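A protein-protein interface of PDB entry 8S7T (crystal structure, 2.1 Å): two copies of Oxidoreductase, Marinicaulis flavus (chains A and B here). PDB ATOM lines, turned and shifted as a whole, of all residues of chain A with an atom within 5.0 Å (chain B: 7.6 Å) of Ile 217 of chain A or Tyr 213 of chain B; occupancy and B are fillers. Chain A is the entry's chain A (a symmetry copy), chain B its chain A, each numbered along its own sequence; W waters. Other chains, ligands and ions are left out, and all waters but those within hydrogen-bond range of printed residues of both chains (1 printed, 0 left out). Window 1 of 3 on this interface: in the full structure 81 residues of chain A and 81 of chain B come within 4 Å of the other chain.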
ATOM      1  N   HIS A 163      14.564  34.479  20.039  1.00  0.00           N
ATOM      2  CA  HIS A 163      13.658  33.340  19.980  1.00  0.00           C
ATOM      3  C   HIS A 163      12.307  33.761  20.535  1.00  0.00           C
ATOM      4  O   HIS A 163      11.601  32.977  21.173  1.00  0.00           O
ATOM      5  CB  HIS A 163      14.222  32.092  20.673  1.00  0.00           C
ATOM      6  CG  HIS A 163      15.527  31.621  20.137  1.00  0.00           C
ATOM      7  ND1 HIS A 163      16.330  30.706  20.781  1.00  0.00           N
ATOM      8  CD2 HIS A 163      16.160  31.939  18.998  1.00  0.00           C
ATOM      9  CE1 HIS A 163      17.431  30.536  20.062  1.00  0.00           C
ATOM     10  NE2 HIS A 163      17.321  31.240  18.963  1.00  0.00           N
ATOM     11  N   PHE A 174      11.841  33.339  14.997  1.00  0.00           N
ATOM     12  CA  PHE A 174      13.124  33.005  14.393  1.00  0.00           C
ATOM     13  C   PHE A 174      12.937  31.925  13.323  1.00  0.00           C
ATOM     14  O   PHE A 174      13.667  31.914  12.341  1.00  0.00           O
ATOM     15  CB  PHE A 174      14.202  32.595  15.405  1.00  0.00           C
ATOM     16  CG  PHE A 174      15.584  32.560  14.791  1.00  0.00           C
ATOM     17  CD1 PHE A 174      16.198  33.720  14.366  1.00  0.00           C
ATOM     18  CD2 PHE A 174      16.203  31.357  14.507  1.00  0.00           C
ATOM     19  CE1 PHE A 174      17.440  33.681  13.749  1.00  0.00           C
ATOM     20  CE2 PHE A 174      17.437  31.314  13.882  1.00  0.00           C
ATOM     21  CZ  PHE A 174      18.054  32.474  13.504  1.00  0.00           C
ATOM     22  N   VAL A 214      24.021  28.540   9.234  1.00  0.00           N
ATOM     23  CA  VAL A 214      24.673  29.253  10.320  1.00  0.00           C
ATOM     24  C   VAL A 214      23.813  30.388  10.899  1.00  0.00           C
ATOM     25  O   VAL A 214      24.196  30.991  11.913  1.00  0.00           O
ATOM     26  CB  VAL A 214      26.035  29.825   9.882  1.00  0.00           C
ATOM     27  CG1 VAL A 214      27.088  28.747   9.693  1.00  0.00           C
ATOM     28  CG2 VAL A 214      25.902  30.731   8.663  1.00  0.00           C
ATOM     29  N   ASP A 215      22.661  30.686  10.303  1.00  0.00           N
ATOM     30  CA  ASP A 215      21.853  31.811  10.764  1.00  0.00           C
ATOM     31  C   ASP A 215      21.578  31.720  12.263  1.00  0.00           C
ATOM     32  O   ASP A 215      21.628  32.730  12.988  1.00  0.00           O
ATOM     33  CB  ASP A 215      20.534  31.916   9.996  1.00  0.00           C
ATOM     34  CG  ASP A 215      20.705  32.343   8.543  1.00  0.00           C
ATOM     35  OD1 ASP A 215      21.298  31.557   7.785  1.00  0.00           O
ATOM     36  OD2 ASP A 215      20.293  33.499   8.197  1.00  0.00           O
ATOM     37  N   GLY A 216      21.253  30.500  12.706  1.00  0.00           N
ATOM     38  CA  GLY A 216      20.930  30.202  14.090  1.00  0.00           C
ATOM     39  C   GLY A 216      22.044  30.547  15.075  1.00  0.00           C
ATOM     40  O   GLY A 216      21.752  30.873  16.211  1.00  0.00           O
ATOM     41  N   ILE A 217      23.309  30.522  14.646  1.00  0.00           N
ATOM     42  CA  ILE A 217      24.382  30.801  15.581  1.00  0.00           C
ATOM     43  C   ILE A 217      24.399  32.285  15.967  1.00  0.00           C
ATOM     44  O   ILE A 217      25.071  32.632  16.930  1.00  0.00           O
ATOM     45  CB  ILE A 217      25.736  30.326  15.042  1.00  0.00           C
ATOM     46  CG1 ILE A 217      26.398  31.352  14.117  1.00  0.00           C
ATOM     47  CG2 ILE A 217      25.619  28.939  14.407  1.00  0.00           C
ATOM     48  CD1 ILE A 217      27.822  31.022  13.845  1.00  0.00           C
ATOM     49  N   PHE A 218      23.627  33.147  15.276  1.00  0.00           N
ATOM     50  CA  PHE A 218      23.576  34.563  15.613  1.00  0.00           C
ATOM     51  C   PHE A 218      22.284  34.910  16.355  1.00  0.00           C
ATOM     52  O   PHE A 218      21.963  36.084  16.544  1.00  0.00           O
ATOM     53  CB  PHE A 218      23.719  35.411  14.345  1.00  0.00           C
ATOM     54  CG  PHE A 218      24.978  35.116  13.574  1.00  0.00           C
ATOM     55  CD1 PHE A 218      26.207  35.517  14.056  1.00  0.00           C
ATOM     56  CD2 PHE A 218      24.938  34.417  12.377  1.00  0.00           C
ATOM     57  CE1 PHE A 218      27.376  35.234  13.366  1.00  0.00           C
ATOM     58  CE2 PHE A 218      26.108  34.130  11.691  1.00  0.00           C
ATOM     59  CZ  PHE A 218      27.327  34.541  12.179  1.00  0.00           C
ATOM     60  N   SER A 219      21.519  33.891  16.749  1.00  0.00           N
ATOM     61  CA  SER A 219      20.364  34.078  17.612  1.00  0.00           C
ATOM     62  C   SER A 219      20.757  33.662  19.028  1.00  0.00           C
ATOM     63  O   SER A 219      21.527  32.713  19.197  1.00  0.00           O
ATOM     64  CB  SER A 219      19.181  33.288  17.103  1.00  0.00           C
ATOM     65  OG  SER A 219      19.456  31.886  17.179  1.00  0.00           O
ATOM     66  N   SER A 221      22.903  35.074  21.008  1.00  0.00           N
ATOM     67  CA  SER A 221      24.319  34.902  20.758  1.00  0.00           C
ATOM     68  C   SER A 221      25.077  36.222  20.838  1.00  0.00           C
ATOM     69  O   SER A 221      24.481  37.285  20.702  1.00  0.00           O
ATOM     70  CB  SER A 221      24.474  34.248  19.409  1.00  0.00           C
ATOM     71  OG  SER A 221      25.816  34.167  19.007  1.00  0.00           O
ATOM     72  N   PHE A 223      27.976  36.157  18.829  1.00  0.00           N
ATOM     73  CA  PHE A 223      28.863  35.742  17.746  1.00  0.00           C
ATOM     74  C   PHE A 223      28.861  36.739  16.588  1.00  0.00           C
ATOM     75  O   PHE A 223      29.687  36.640  15.674  1.00  0.00           O
ATOM     76  CB  PHE A 223      28.485  34.365  17.201  1.00  0.00           C
ATOM     77  CG  PHE A 223      28.697  33.216  18.145  1.00  0.00           C
ATOM     78  CD1 PHE A 223      29.372  33.376  19.338  1.00  0.00           C
ATOM     79  CD2 PHE A 223      28.195  31.965  17.838  1.00  0.00           C
ATOM     80  CE1 PHE A 223      29.558  32.295  20.192  1.00  0.00           C
ATOM     81  CE2 PHE A 223      28.380  30.889  18.696  1.00  0.00           C
ATOM     82  CZ  PHE A 223      29.047  31.061  19.880  1.00  0.00           C
ATOM     83  N   ILE A 496      33.775  28.407  19.539  1.00  0.00           N
ATOM     84  CA  ILE A 496      33.353  29.247  18.430  1.00  0.00           C
ATOM     85  C   ILE A 496      33.541  30.718  18.808  1.00  0.00           C
ATOM     86  O   ILE A 496      34.021  31.521  18.007  1.00  0.00           O
ATOM     87  CB  ILE A 496      31.897  28.912  18.022  1.00  0.00           C
ATOM     88  CG1 ILE A 496      31.782  27.460  17.555  1.00  0.00           C
ATOM     89  CG2 ILE A 496      31.410  29.860  16.945  1.00  0.00           C
ATOM     90  CD1 ILE A 496      30.382  26.960  17.376  1.00  0.00           C
ATOM     91  N   LEU A 500      35.725  33.394  16.581  1.00  0.00           N
ATOM     92  CA  LEU A 500      35.116  34.522  15.903  1.00  0.00           C
ATOM     93  C   LEU A 500      35.455  35.830  16.610  1.00  0.00           C
ATOM     94  O   LEU A 500      35.523  36.856  15.941  1.00  0.00           O
ATOM     95  CB  LEU A 500      33.600  34.320  15.874  1.00  0.00           C
ATOM     96  CG  LEU A 500      33.107  33.164  15.003  1.00  0.00           C
ATOM     97  CD1 LEU A 500      31.587  33.041  15.102  1.00  0.00           C
ATOM     98  CD2 LEU A 500      33.529  33.374  13.565  1.00  0.00           C
ATOM     99  N   PHE B 174      15.379  18.725   6.817  1.00  0.00           N
ATOM    100  CA  PHE B 174      16.185  19.307   7.882  1.00  0.00           C
ATOM    101  C   PHE B 174      15.334  20.263   8.724  1.00  0.00           C
ATOM    102  O   PHE B 174      15.567  20.388   9.918  1.00  0.00           O
ATOM    103  CB  PHE B 174      17.464  19.996   7.392  1.00  0.00           C
ATOM    104  CG  PHE B 174      18.420  20.307   8.522  1.00  0.00           C
ATOM    105  CD1 PHE B 174      19.043  19.294   9.221  1.00  0.00           C
ATOM    106  CD2 PHE B 174      18.579  21.603   8.978  1.00  0.00           C
ATOM    107  CE1 PHE B 174      19.873  19.578  10.296  1.00  0.00           C
ATOM    108  CE2 PHE B 174      19.398  21.889  10.057  1.00  0.00           C
ATOM    109  CZ  PHE B 174      20.043  20.877  10.714  1.00  0.00           C
ATOM    110  N   ALA B 175      14.298  20.873   8.136  1.00  0.00           N
ATOM    111  CA  ALA B 175      13.376  21.693   8.929  1.00  0.00           C
ATOM    112  C   ALA B 175      12.670  20.857   9.992  1.00  0.00           C
ATOM    113  O   ALA B 175      12.318  21.387  11.035  1.00  0.00           O
ATOM    114  CB  ALA B 175      12.373  22.400   8.044  1.00  0.00           C
ATOM    115  N   GLN B 177      13.971  18.354  11.538  1.00  0.00           N
ATOM    116  CA  GLN B 177      14.976  17.817  12.443  1.00  0.00           C
ATOM    117  C   GLN B 177      14.778  18.460  13.807  1.00  0.00           C
ATOM    118  O   GLN B 177      14.472  19.644  13.912  1.00  0.00           O
ATOM    119  CB  GLN B 177      16.393  18.066  11.913  1.00  0.00           C
ATOM    120  CG  GLN B 177      17.498  17.564  12.829  1.00  0.00           C
ATOM    121  CD  GLN B 177      18.014  18.650  13.729  1.00  0.00           C
ATOM    122  OE1 GLN B 177      17.906  19.831  13.416  1.00  0.00           O
ATOM    123  NE2 GLN B 177      18.575  18.262  14.856  1.00  0.00           N
ATOM    124  N   CYS B 178      14.963  17.678  14.870  1.00  0.00           N
ATOM    125  CA  CYS B 178      14.831  18.226  16.212  1.00  0.00           C
ATOM    126  C   CYS B 178      15.720  17.454  17.180  1.00  0.00           C
ATOM    127  O   CYS B 178      15.445  16.289  17.506  1.00  0.00           O
ATOM    128  CB  CYS B 178      13.379  18.208  16.667  1.00  0.00           C
ATOM    129  SG  CYS B 178      13.134  19.186  18.166  1.00  0.00           S
ATOM    130  N   GLY B 179      16.806  18.118  17.567  1.00  0.00           N
ATOM    131  CA  GLY B 179      17.810  17.561  18.452  1.00  0.00           C
ATOM    132  C   GLY B 179      18.777  16.630  17.723  1.00  0.00           C
ATOM    133  O   GLY B 179      18.359  15.888  16.832  1.00  0.00           O
ATOM    134  N   MET B 180      20.066  16.687  18.111  1.00  0.00           N
ATOM    135  CA  MET B 180      21.056  15.766  17.569  1.00  0.00           C
ATOM    136  C   MET B 180      22.188  15.547  18.576  1.00  0.00           C
ATOM    137  O   MET B 180      22.457  16.370  19.459  1.00  0.00           O
ATOM    138  CB  MET B 180      21.616  16.240  16.222  1.00  0.00           C
ATOM    139  CG  MET B 180      22.336  17.572  16.285  1.00  0.00           C
ATOM    140  SD  MET B 180      23.191  18.050  14.768  1.00  0.00           S
ATOM    141  CE  MET B 180      21.832  18.030  13.594  1.00  0.00           C
ATOM    142  N   THR B 192      22.627  18.803  21.189  1.00  0.00           N
ATOM    143  CA  THR B 192      22.068  20.106  20.910  1.00  0.00           C
ATOM    144  C   THR B 192      20.698  20.217  21.570  1.00  0.00           C
ATOM    145  O   THR B 192      20.105  19.205  21.952  1.00  0.00           O
ATOM    146  CB  THR B 192      21.972  20.331  19.400  1.00  0.00           C
ATOM    147  OG1 THR B 192      20.968  19.437  18.933  1.00  0.00           O
ATOM    148  CG2 THR B 192      23.288  20.092  18.701  1.00  0.00           C
ATOM    149  N   GLY B 193      20.217  21.471  21.664  1.00  0.00           N
ATOM    150  CA  GLY B 193      18.862  21.750  22.101  1.00  0.00           C
ATOM    151  C   GLY B 193      18.658  21.305  23.547  1.00  0.00           C
ATOM    152  O   GLY B 193      19.519  21.477  24.414  1.00  0.00           O
ATOM    153  N   PHE B 206      11.365  20.460  21.033  1.00  0.00           N
ATOM    154  CA  PHE B 206      11.668  21.876  20.960  1.00  0.00           C
ATOM    155  C   PHE B 206      13.081  22.017  20.409  1.00  0.00           C
ATOM    156  O   PHE B 206      14.026  21.538  21.033  1.00  0.00           O
ATOM    157  CB  PHE B 206      11.476  22.506  22.350  1.00  0.00           C
ATOM    158  CG  PHE B 206      11.729  23.995  22.432  1.00  0.00           C
ATOM    159  CD1 PHE B 206      10.795  24.901  21.963  1.00  0.00           C
ATOM    160  CD2 PHE B 206      12.918  24.488  22.944  1.00  0.00           C
ATOM    161  CE1 PHE B 206      11.037  26.266  22.027  1.00  0.00           C
ATOM    162  CE2 PHE B 206      13.158  25.854  22.996  1.00  0.00           C
ATOM    163  CZ  PHE B 206      12.215  26.740  22.553  1.00  0.00           C
ATOM    164  N   LYS B 207      13.211  22.731  19.286  1.00  0.00           N
ATOM    165  CA  LYS B 207      14.445  22.717  18.522  1.00  0.00           C
ATOM    166  C   LYS B 207      15.558  23.455  19.241  1.00  0.00           C
ATOM    167  O   LYS B 207      16.713  23.016  19.235  1.00  0.00           O
ATOM    168  CB  LYS B 207      14.291  23.415  17.174  1.00  0.00           C
ATOM    169  CG  LYS B 207      13.584  22.645  16.073  1.00  0.00           C
ATOM    170  CD  LYS B 207      13.346  23.549  14.900  1.00  0.00           C
ATOM    171  CE  LYS B 207      12.972  22.847  13.624  1.00  0.00           C
ATOM    172  NZ  LYS B 207      14.162  22.218  13.015  1.00  0.00           N
ATOM    173  N   TYR B 208      15.227  24.629  19.786  1.00  0.00           N
ATOM    174  CA  TYR B 208      16.281  25.577  20.091  1.00  0.00           C
ATOM    175  C   TYR B 208      17.130  25.168  21.283  1.00  0.00           C
ATOM    176  O   TYR B 208      18.325  25.444  21.275  1.00  0.00           O
ATOM    177  CB  TYR B 208      15.727  26.985  20.320  1.00  0.00           C
ATOM    178  CG  TYR B 208      14.984  27.558  19.149  1.00  0.00           C
ATOM    179  CD1 TYR B 208      15.519  27.554  17.873  1.00  0.00           C
ATOM    180  CD2 TYR B 208      13.720  28.089  19.317  1.00  0.00           C
ATOM    181  CE1 TYR B 208      14.816  28.072  16.798  1.00  0.00           C
ATOM    182  CE2 TYR B 208      13.010  28.621  18.259  1.00  0.00           C
ATOM    183  CZ  TYR B 208      13.565  28.629  16.997  1.00  0.00           C
ATOM    184  OH  TYR B 208      12.831  29.189  15.986  1.00  0.00           O
ATOM    185  N   GLY B 209      16.519  24.569  22.314  1.00  0.00           N
ATOM    186  CA  GLY B 209      17.059  24.706  23.653  1.00  0.00           C
ATOM    187  C   GLY B 209      17.286  26.185  24.006  1.00  0.00           C
ATOM    188  O   GLY B 209      16.414  27.020  23.798  1.00  0.00           O
ATOM    189  N   TYR B 210      18.477  26.511  24.521  1.00  0.00           N
ATOM    190  CA  TYR B 210      18.807  27.879  24.891  1.00  0.00           C
ATOM    191  C   TYR B 210      20.168  28.237  24.313  1.00  0.00           C
ATOM    192  O   TYR B 210      21.055  27.391  24.252  1.00  0.00           O
ATOM    193  CB  TYR B 210      18.807  27.985  26.420  1.00  0.00           C
ATOM    194  CG  TYR B 210      19.415  29.216  27.037  1.00  0.00           C
ATOM    195  CD1 TYR B 210      18.761  30.436  27.000  1.00  0.00           C
ATOM    196  CD2 TYR B 210      20.634  29.151  27.698  1.00  0.00           C
ATOM    197  CE1 TYR B 210      19.308  31.568  27.576  1.00  0.00           C
ATOM    198  CE2 TYR B 210      21.191  30.272  28.290  1.00  0.00           C
ATOM    199  CZ  TYR B 210      20.520  31.479  28.228  1.00  0.00           C
ATOM    200  OH  TYR B 210      21.043  32.580  28.835  1.00  0.00           O
ATOM    201  N   GLY B 211      20.334  29.505  23.929  1.00  0.00           N
ATOM    202  CA  GLY B 211      21.611  29.989  23.443  1.00  0.00           C
ATOM    203  C   GLY B 211      21.677  29.880  21.920  1.00  0.00           C
ATOM    204  O   GLY B 211      20.658  29.690  21.259  1.00  0.00           O
ATOM    205  N   PRO B 212      22.879  29.956  21.337  1.00  0.00           N
ATOM    206  CA  PRO B 212      23.038  29.875  19.886  1.00  0.00           C
ATOM    207  C   PRO B 212      22.445  28.588  19.315  1.00  0.00           C
ATOM    208  O   PRO B 212      22.600  27.498  19.871  1.00  0.00           O
ATOM    209  CB  PRO B 212      24.555  29.936  19.662  1.00  0.00           C
ATOM    210  CG  PRO B 212      25.134  30.454  20.942  1.00  0.00           C
ATOM    211  CD  PRO B 212      24.145  30.126  22.040  1.00  0.00           C
ATOM    212  N   TYR B 213      21.764  28.721  18.182  1.00  0.00           N
ATOM    213  CA  TYR B 213      21.098  27.580  17.582  1.00  0.00           C
ATOM    214  C   TYR B 213      22.061  26.989  16.565  1.00  0.00           C
ATOM    215  O   TYR B 213      22.325  27.632  15.567  1.00  0.00           O
ATOM    216  CB  TYR B 213      19.759  28.033  16.997  1.00  0.00           C
ATOM    217  CG  TYR B 213      19.025  26.939  16.272  1.00  0.00           C
ATOM    218  CD1 TYR B 213      18.986  25.662  16.796  1.00  0.00           C
ATOM    219  CD2 TYR B 213      18.338  27.184  15.089  1.00  0.00           C
ATOM    220  CE1 TYR B 213      18.337  24.632  16.143  1.00  0.00           C
ATOM    221  CE2 TYR B 213      17.668  26.169  14.432  1.00  0.00           C
ATOM    222  CZ  TYR B 213      17.692  24.882  14.952  1.00  0.00           C
ATOM    223  OH  TYR B 213      17.068  23.825  14.366  1.00  0.00           O
ATOM    224  N   VAL B 214      22.652  25.827  16.880  1.00  0.00           N
ATOM    225  CA  VAL B 214      23.838  25.331  16.200  1.00  0.00           C
ATOM    226  C   VAL B 214      23.573  24.063  15.373  1.00  0.00           C
ATOM    227  O   VAL B 214      24.466  23.611  14.641  1.00  0.00           O
ATOM    228  CB  VAL B 214      24.984  25.056  17.192  1.00  0.00           C
ATOM    229  CG1 VAL B 214      25.593  26.331  17.749  1.00  0.00           C
ATOM    230  CG2 VAL B 214      24.561  24.085  18.288  1.00  0.00           C
ATOM    231  N   ASP B 215      22.375  23.487  15.449  1.00  0.00           N
ATOM    232  CA  ASP B 215      22.105  22.234  14.750  1.00  0.00           C
ATOM    233  C   ASP B 215      22.467  22.336  13.270  1.00  0.00           C
ATOM    234  O   ASP B 215      23.037  21.399  12.682  1.00  0.00           O
ATOM    235  CB  ASP B 215      20.646  21.801  14.904  1.00  0.00           C
ATOM    236  CG  ASP B 215      20.288  21.351  16.315  1.00  0.00           C
ATOM    237  OD1 ASP B 215      20.320  22.211  17.212  1.00  0.00           O
ATOM    238  OD2 ASP B 215      20.039  20.117  16.515  1.00  0.00           O
ATOM    239  N   GLY B 216      22.092  23.473  12.672  1.00  0.00           N
ATOM    240  CA  GLY B 216      22.317  23.760  11.266  1.00  0.00           C
ATOM    241  C   GLY B 216      23.786  23.720  10.852  1.00  0.00           C
ATOM    242  O   GLY B 216      24.073  23.394   9.716  1.00  0.00           O
ATOM    243  N   ILE B 217      24.717  24.005  11.767  1.00  0.00           N
ATOM    244  CA  ILE B 217      26.114  24.018  11.378  1.00  0.00           C
ATOM    245  C   ILE B 217      26.620  22.596  11.108  1.00  0.00           C
ATOM    246  O   ILE B 217      27.690  22.455  10.530  1.00  0.00           O
ATOM    247  CB  ILE B 217      26.978  24.756  12.407  1.00  0.00           C
ATOM    248  CG1 ILE B 217      27.405  23.859  13.573  1.00  0.00           C
ATOM    249  CG2 ILE B 217      26.302  26.049  12.867  1.00  0.00           C
ATOM    250  CD1 ILE B 217      28.474  24.483  14.396  1.00  0.00           C
ATOM    251  N   TRP B 232      10.690  15.090  13.224  1.00  0.00           N
ATOM    252  CA  TRP B 232       9.277  15.155  13.473  1.00  0.00           C
ATOM    253  C   TRP B 232       8.589  14.332  12.410  1.00  0.00           C
ATOM    254  O   TRP B 232       9.002  14.371  11.250  1.00  0.00           O
ATOM    255  CB  TRP B 232       8.785  16.606  13.478  1.00  0.00           C
ATOM    256  CG  TRP B 232       9.276  17.409  14.646  1.00  0.00           C
ATOM    257  CD1 TRP B 232       9.695  16.950  15.859  1.00  0.00           C
ATOM    258  CD2 TRP B 232       9.451  18.833  14.683  1.00  0.00           C
ATOM    259  NE1 TRP B 232      10.096  17.988  16.651  1.00  0.00           N
ATOM    260  CE2 TRP B 232       9.972  19.153  15.948  1.00  0.00           C
ATOM    261  CE3 TRP B 232       9.201  19.862  13.772  1.00  0.00           C
ATOM    262  CZ2 TRP B 232      10.204  20.467  16.351  1.00  0.00           C
ATOM    263  CZ3 TRP B 232       9.460  21.161  14.158  1.00  0.00           C
ATOM    264  CH2 TRP B 232       9.972  21.453  15.429  1.00  0.00           C
ATOM    265  N   MET B 492      34.346  32.594   6.921  1.00  0.00           N
ATOM    266  CA  MET B 492      33.783  32.327   8.226  1.00  0.00           C
ATOM    267  C   MET B 492      33.665  30.822   8.450  1.00  0.00           C
ATOM    268  O   MET B 492      34.050  30.342   9.516  1.00  0.00           O
ATOM    269  CB  MET B 492      32.405  32.958   8.411  1.00  0.00           C
ATOM    270  CG  MET B 492      31.956  32.946   9.875  1.00  0.00           C
ATOM    271  SD  MET B 492      30.216  33.389  10.017  1.00  0.00           S
ATOM    272  CE  MET B 492      29.480  31.833   9.534  1.00  0.00           C
ATOM    273  N   ILE B 496      35.509  28.636  11.572  1.00  0.00           N
ATOM    274  CA  ILE B 496      34.862  27.670  12.446  1.00  0.00           C
ATOM    275  C   ILE B 496      35.513  26.298  12.253  1.00  0.00           C
ATOM    276  O   ILE B 496      35.782  25.584  13.220  1.00  0.00           O
ATOM    277  CB  ILE B 496      33.334  27.652  12.194  1.00  0.00           C
ATOM    278  CG1 ILE B 496      32.716  29.017  12.498  1.00  0.00           C
ATOM    279  CG2 ILE B 496      32.669  26.567  13.016  1.00  0.00           C
ATOM    280  CD1 ILE B 496      31.295  29.183  12.054  1.00  0.00           C
HETATM  281  O   HOH W   1      15.858  29.430  22.950  1.00  0.00           O
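Of the printed residues of chain B, Phe 174 of chain A touches Tyr 208.
Of the printed residues of chain B, Ile 217 of chain A touches Pro 212 (3.9 Å), Tyr 213 (3.2 Å) and Ile 217 (3.3 Å).
Of the printed residues of chain B, Ser 219 of chain A touches Gly 211, Pro 212 and Tyr 213.
Of the printed residues of chain A, Tyr 208 of chain B touches His 163 and Phe 174.
Of the printed residues of chain A, Gly 211 of chain B touches His 163 and Ser 219.
Tyr 213 of chain B touches just these residues of chain A: Gly 216 (2.9 Å), Ile 217 (3.2 Å) and Ser 219 (3.9 Å).
The nearest residue of chain B that does not touch Ile 217 of chain A is Val 214 of chain B (4.2 Å).
The nearest residue of chain A that does not touch Tyr 213 of chain B is Phe 174 of chain A (4.4 Å).
Tyr 208 of chain B touches His 163 of chain A (CG to ND1, 3.8 Å).
CE1 of His 163 of chain A touches O of Gly 211 of chain B (3.5 Å).
OH of Tyr 208 of chain B touches CB of Phe 174 of chain A, at 3.7 Å.
Val 214 of chain A touches Met 492 of chain B (CG2 to CE, 3.8 Å).
Gly 216 of chain A touches Pro 212 of chain B (O to C, 3.9 Å).
CG2 of Ile 217 of chain A touches CG2 of Ile 217 of chain B, 3.3 Å away.
Phe 218 of chain A touches Met 492 of chain B.
O of Gly 211 of chain B touches O of Ser 219 of chain A, at 3.8 Å.
O of Ser 219 of chain A touches CA of Pro 212 of chain B, 3.3 Å away.
Tyr 213 of chain B touches Ser 219 of chain A (CB to OG, 3.9 Å).
Water W1 lies within hydrogen-bond range of ND1 of His 163 of chain A (2.6 Å) and O of Gly 209 of chain B (2.6 Å).
A ring nitrogen (NE2) of His 163 of chain A sits at hydrogen-bond distance from the side-chain hydroxyl of Ser 219 of chain A, at 2.9 Å.
O of Gly 216 of chain A lies within hydrogen-bond range of OG of Ser 219 of chain A (2.7 Å).
The backbone carbonyl oxygen (O) of Ile 217 of chain A is in hydrogen-bond range of the side-chain hydroxyl (OG) of Ser 221 of chain A (2.7 Å).
The backbone NH of Phe 223 of chain A is in hydrogen-bond range of the side-chain hydroxyl of Ser 221 of chain A (2.9 Å).
O of Gly 216 of chain A lies within hydrogen-bond range of N of Tyr 213 of chain B (2.9 Å).
The backbone carbonyl oxygen (O) of Tyr 213 of chain B sits at hydrogen-bond distance from the backbone NH (N) of Ile 217 of chain A.
Ile 217 of chain B touches its own counterpart, Ile 217 of chain A.
Of the 23 printed residues of chain B, 6 touch a printed residue of chain A.
Printed residues of chain B that touch a printed residue of chain A: Tyr 208, Gly 211, Pro 212, Tyr 213, Ile 217 and Met 492.
Hydrophobic or aromatic side chains of chain B that line the printed part of chain A: Tyr 208, Pro 212, Tyr 213, Ile 217 and Met 492.
Among the printed residues, 14 pairs touch across the chains.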
